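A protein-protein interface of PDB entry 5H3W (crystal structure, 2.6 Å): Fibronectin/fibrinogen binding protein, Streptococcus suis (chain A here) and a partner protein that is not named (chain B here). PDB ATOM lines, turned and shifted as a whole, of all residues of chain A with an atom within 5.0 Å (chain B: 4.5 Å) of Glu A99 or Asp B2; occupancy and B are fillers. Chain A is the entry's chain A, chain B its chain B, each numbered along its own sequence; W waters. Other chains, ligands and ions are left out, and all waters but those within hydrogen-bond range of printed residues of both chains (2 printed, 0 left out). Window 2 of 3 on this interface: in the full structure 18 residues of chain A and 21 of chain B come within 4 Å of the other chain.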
ATOM      1  N   GLN A  95      -7.761  10.614   2.640  1.00  0.00           N
ATOM      2  CA  GLN A  95      -6.934   9.880   1.688  1.00  0.00           C
ATOM      3  C   GLN A  95      -5.470  10.268   1.958  1.00  0.00           C
ATOM      4  O   GLN A  95      -4.555   9.432   1.865  1.00  0.00           O
ATOM      5  CB  GLN A  95      -7.333  10.164   0.231  1.00  0.00           C
ATOM      6  CG  GLN A  95      -6.235  10.837  -0.606  1.00  0.00           C
ATOM      7  CD  GLN A  95      -5.853  10.066  -1.865  1.00  0.00           C
ATOM      8  OE1 GLN A  95      -6.189  10.478  -2.991  1.00  0.00           O
ATOM      9  NE2 GLN A  95      -5.136   8.952  -1.687  1.00  0.00           N
ATOM     10  N   LYS A  96      -5.257  11.528   2.331  1.00  0.00           N
ATOM     11  CA  LYS A  96      -3.912  12.013   2.590  1.00  0.00           C
ATOM     12  C   LYS A  96      -3.359  11.436   3.897  1.00  0.00           C
ATOM     13  O   LYS A  96      -2.184  11.098   3.986  1.00  0.00           O
ATOM     14  CB  LYS A  96      -3.912  13.544   2.632  1.00  0.00           C
ATOM     15  CG  LYS A  96      -4.091  14.202   1.252  1.00  0.00           C
ATOM     16  CD  LYS A  96      -3.825  15.703   1.277  1.00  0.00           C
ATOM     17  CE  LYS A  96      -2.325  15.993   1.166  1.00  0.00           C
ATOM     18  NZ  LYS A  96      -2.012  17.368   0.646  1.00  0.00           N
ATOM     19  N   LEU A  97      -4.222  11.277   4.897  1.00  0.00           N
ATOM     20  CA  LEU A  97      -3.792  10.761   6.192  1.00  0.00           C
ATOM     21  C   LEU A  97      -3.442   9.293   5.992  1.00  0.00           C
ATOM     22  O   LEU A  97      -2.464   8.784   6.536  1.00  0.00           O
ATOM     23  CB  LEU A  97      -4.896  10.944   7.226  1.00  0.00           C
ATOM     24  CG  LEU A  97      -5.144  12.398   7.616  1.00  0.00           C
ATOM     25  CD1 LEU A  97      -6.483  12.522   8.327  1.00  0.00           C
ATOM     26  CD2 LEU A  97      -3.990  12.962   8.436  1.00  0.00           C
ATOM     27  N   LYS A  98      -4.247   8.634   5.164  1.00  0.00           N
ATOM     28  CA  LYS A  98      -4.062   7.225   4.834  1.00  0.00           C
ATOM     29  C   LYS A  98      -2.758   6.960   4.059  1.00  0.00           C
ATOM     30  O   LYS A  98      -2.187   5.873   4.177  1.00  0.00           O
ATOM     31  CB  LYS A  98      -5.274   6.723   4.049  1.00  0.00           C
ATOM     32  CG  LYS A  98      -5.378   5.233   3.864  1.00  0.00           C
ATOM     33  CD  LYS A  98      -6.640   4.939   3.076  1.00  0.00           C
ATOM     34  CE  LYS A  98      -6.504   3.679   2.252  1.00  0.00           C
ATOM     35  NZ  LYS A  98      -7.376   3.792   1.051  1.00  0.00           N
ATOM     36  N   GLU A  99      -2.273   7.946   3.297  1.00  0.00           N
ATOM     37  CA  GLU A  99      -1.020   7.789   2.551  1.00  0.00           C
ATOM     38  C   GLU A  99       0.150   7.862   3.521  1.00  0.00           C
ATOM     39  O   GLU A  99       1.137   7.133   3.379  1.00  0.00           O
ATOM     40  CB  GLU A  99      -0.837   8.881   1.464  1.00  0.00           C
ATOM     41  CG  GLU A  99      -1.433   8.603   0.055  1.00  0.00           C
ATOM     42  CD  GLU A  99      -1.125   7.198  -0.508  1.00  0.00           C
ATOM     43  OE1 GLU A  99       0.068   6.845  -0.636  1.00  0.00           O
ATOM     44  OE2 GLU A  99      -2.074   6.440  -0.844  1.00  0.00           O
ATOM     45  N   ALA A 100       0.063   8.779   4.480  1.00  0.00           N
ATOM     46  CA  ALA A 100       1.095   8.892   5.509  1.00  0.00           C
ATOM     47  C   ALA A 100       1.158   7.594   6.355  1.00  0.00           C
ATOM     48  O   ALA A 100       2.251   7.124   6.697  1.00  0.00           O
ATOM     49  CB  ALA A 100       0.854  10.129   6.375  1.00  0.00           C
ATOM     50  N   VAL A 101       0.000   7.027   6.691  1.00  0.00           N
ATOM     51  CA  VAL A 101      -0.050   5.742   7.390  1.00  0.00           C
ATOM     52  C   VAL A 101       0.721   4.672   6.601  1.00  0.00           C
ATOM     53  O   VAL A 101       1.509   3.895   7.169  1.00  0.00           O
ATOM     54  CB  VAL A 101      -1.521   5.262   7.609  1.00  0.00           C
ATOM     55  CG1 VAL A 101      -1.577   3.794   7.979  1.00  0.00           C
ATOM     56  CG2 VAL A 101      -2.229   6.098   8.651  1.00  0.00           C
ATOM     57  N   LYS A 102       0.489   4.635   5.289  1.00  0.00           N
ATOM     58  CA  LYS A 102       1.219   3.730   4.398  1.00  0.00           C
ATOM     59  C   LYS A 102       2.733   4.009   4.439  1.00  0.00           C
ATOM     60  O   LYS A 102       3.542   3.082   4.512  1.00  0.00           O
ATOM     61  CB  LYS A 102       0.715   3.879   2.973  1.00  0.00           C
ATOM     62  CG  LYS A 102      -0.188   2.791   2.520  1.00  0.00           C
ATOM     63  CD  LYS A 102      -1.491   3.367   1.999  1.00  0.00           C
ATOM     64  CE  LYS A 102      -1.443   3.556   0.510  1.00  0.00           C
ATOM     65  NZ  LYS A 102      -2.798   3.575  -0.084  1.00  0.00           N
ATOM     66  N   HIS A 103       3.118   5.281   4.395  1.00  0.00           N
ATOM     67  CA  HIS A 103       4.534   5.629   4.435  1.00  0.00           C
ATOM     68  C   HIS A 103       5.125   5.168   5.746  1.00  0.00           C
ATOM     69  O   HIS A 103       6.185   4.523   5.780  1.00  0.00           O
ATOM     70  CB  HIS A 103       4.743   7.131   4.285  1.00  0.00           C
ATOM     71  CG  HIS A 103       6.182   7.546   4.282  1.00  0.00           C
ATOM     72  ND1 HIS A 103       7.106   7.040   3.381  1.00  0.00           N
ATOM     73  CD2 HIS A 103       6.854   8.441   5.043  1.00  0.00           C
ATOM     74  CE1 HIS A 103       8.287   7.587   3.610  1.00  0.00           C
ATOM     75  NE2 HIS A 103       8.163   8.440   4.612  1.00  0.00           N
ATOM     76  N   ARG B   1      -3.808  11.345  -4.698  1.00  0.00           N
ATOM     77  CA  ARG B   1      -3.057  10.221  -5.255  1.00  0.00           C
ATOM     78  C   ARG B   1      -2.762   9.105  -4.250  1.00  0.00           C
ATOM     79  O   ARG B   1      -2.413   9.352  -3.078  1.00  0.00           O
ATOM     80  CB  ARG B   1      -1.749  10.683  -5.907  1.00  0.00           C
ATOM     81  CG  ARG B   1      -1.752  10.712  -7.436  1.00  0.00           C
ATOM     82  CD  ARG B   1      -1.788   9.315  -8.044  1.00  0.00           C
ATOM     83  NE  ARG B   1      -3.089   8.666  -7.871  1.00  0.00           N
ATOM     84  CZ  ARG B   1      -3.482   7.592  -8.544  1.00  0.00           C
ATOM     85  NH1 ARG B   1      -2.671   7.043  -9.438  1.00  0.00           N
ATOM     86  NH2 ARG B   1      -4.683   7.074  -8.328  1.00  0.00           N
ATOM     87  N   ASP B   2      -2.892   7.877  -4.748  1.00  0.00           N
ATOM     88  CA  ASP B   2      -2.706   6.673  -3.959  1.00  0.00           C
ATOM     89  C   ASP B   2      -1.402   5.991  -4.336  1.00  0.00           C
ATOM     90  O   ASP B   2      -1.254   4.788  -4.169  1.00  0.00           O
ATOM     91  CB  ASP B   2      -3.886   5.726  -4.188  1.00  0.00           C
ATOM     92  CG  ASP B   2      -5.234   6.434  -4.074  1.00  0.00           C
ATOM     93  OD1 ASP B   2      -5.796   6.834  -5.124  1.00  0.00           O
ATOM     94  OD2 ASP B   2      -5.726   6.592  -2.930  1.00  0.00           O
ATOM     95  N   ARG B   3      -0.468   6.775  -4.861  1.00  0.00           N
ATOM     96  CA  ARG B   3       0.866   6.300  -5.218  1.00  0.00           C
ATOM     97  C   ARG B   3       1.935   7.102  -4.486  1.00  0.00           C
ATOM     98  O   ARG B   3       3.126   6.776  -4.536  1.00  0.00           O
ATOM     99  CB  ARG B   3       1.099   6.357  -6.728  1.00  0.00           C
ATOM    100  CG  ARG B   3       0.350   5.302  -7.548  1.00  0.00           C
ATOM    101  CD  ARG B   3       1.038   5.111  -8.893  1.00  0.00           C
ATOM    102  NE  ARG B   3       0.096   4.847  -9.974  1.00  0.00           N
ATOM    103  CZ  ARG B   3      -0.297   5.771 -10.845  1.00  0.00           C
ATOM    104  NH1 ARG B   3       0.143   7.015 -10.716  1.00  0.00           N
ATOM    105  NH2 ARG B   3      -1.156   5.471 -11.811  1.00  0.00           N
ATOM    106  N   VAL B   4       1.497   8.157  -3.806  1.00  0.00           N
ATOM    107  CA  VAL B   4       2.410   9.058  -3.120  1.00  0.00           C
ATOM    108  C   VAL B   4       3.401   8.330  -2.199  1.00  0.00           C
ATOM    109  O   VAL B   4       4.612   8.526  -2.340  1.00  0.00           O
ATOM    110  CB  VAL B   4       1.643  10.158  -2.376  1.00  0.00           C
ATOM    111  CG1 VAL B   4       2.584  11.000  -1.496  1.00  0.00           C
ATOM    112  CG2 VAL B   4       0.907  11.021  -3.384  1.00  0.00           C
ATOM    113  N   ALA B   5       2.906   7.464  -1.312  1.00  0.00           N
ATOM    114  CA  ALA B   5       3.780   6.706  -0.409  1.00  0.00           C
ATOM    115  C   ALA B   5       4.591   5.662  -1.162  1.00  0.00           C
ATOM    116  O   ALA B   5       5.751   5.439  -0.869  1.00  0.00           O
ATOM    117  CB  ALA B   5       2.970   6.045   0.715  1.00  0.00           C
ATOM    118  N   LEU B 131       5.860  13.027   4.000  1.00  0.00           N
ATOM    119  CA  LEU B 131       5.670  12.891   2.556  1.00  0.00           C
ATOM    120  C   LEU B 131       5.865  14.236   1.853  1.00  0.00           C
ATOM    121  O   LEU B 131       6.430  14.305   0.757  1.00  0.00           O
ATOM    122  CB  LEU B 131       4.281  12.312   2.249  1.00  0.00           C
ATOM    123  CG  LEU B 131       4.148  10.834   2.638  1.00  0.00           C
ATOM    124  CD1 LEU B 131       2.721  10.299   2.440  1.00  0.00           C
ATOM    125  CD2 LEU B 131       5.153  10.009   1.843  1.00  0.00           C
HETATM  126  O   HOH W   1       6.775   4.943   1.922  1.00  0.00           O
HETATM  127  O   HOH W   2       1.110   4.643  -1.892  1.00  0.00           O
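The side-chain carboxylate of Asp B2 lies within salt-bridge range of the guanidinium group of Arg B1 (3.4 Å).
The side-chain carboxylate (OE2) of Glu A99 lies within salt-bridge range of the side-chain amino group (NZ) of Lys A102 (3.1 Å).
Printed residues of chain A within 4 Å of Leu B131: Glu A99 (3.7 Å), Ala A100 (3.7 Å) and His A103 (3.6 Å).
Of the printed residues of chain B, Gln A95 touches Arg B1 (3.1 Å) and Asp B2 (2.7 Å).
Of the printed residues of chain B, His A103 touches Ala B5 (3.8 Å) and Leu B131 (3.6 Å).
Of the printed residues of chain A, Arg B1 touches Gln A95 and Glu A99.
Of the printed residues of chain A, Val B4 touches Glu A99.
Val A101 touches none of the printed residues of chain B.
Lys A96 touches none of the printed residues of chain B.
Glu A99 touches Arg B1 (CG to O, 3.4 Å).
Glu A99 touches Asp B2 (OE2 to CA, 3.2 Å).
Val B4 touches Glu A99.
Leu B131 touches Glu A99.
Ala A100 touches Leu B131 (N to CD1, 3.7 Å).
CB of Lys A102 touches CB of Ala B5 (3.9 Å).
Ala B5 touches His A103.
His A103 touches Leu B131.
N of Arg B1 sits at hydrogen-bond distance from OE1 of Gln A95, 3.1 Å away.
The side-chain carboxylate of Asp B2 is in hydrogen-bond range of the side-chain amide nitrogen of Gln A95, at 2.7 Å.
OE1 of Glu A99 sits at hydrogen-bond distance from N of Ala B5 (3.0 Å).
Printed residues of chain A that touch a printed residue of chain B: Gln A95, Glu A99, Ala A100, Lys A102 and His A103.
Of the 6 printed residues of chain B, 5 touch a printed residue of chain A.
Hydrophobic or aromatic side chains of chain B within 4 Å of the printed part of chain A: Ala B5 and Leu B131.
Water W1 lies within hydrogen-bond range of a ring nitrogen (ND1) of His A103 (2.6 Å) and the backbone carbonyl oxygen of Ala B5 (3.0 Å).
Water W2 lies within hydrogen-bond range of the side-chain carboxylate (OE1) of Glu A99, the backbone carbonyl oxygen (O) of Asp B2 and the backbone NH (N) of Ala B5.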
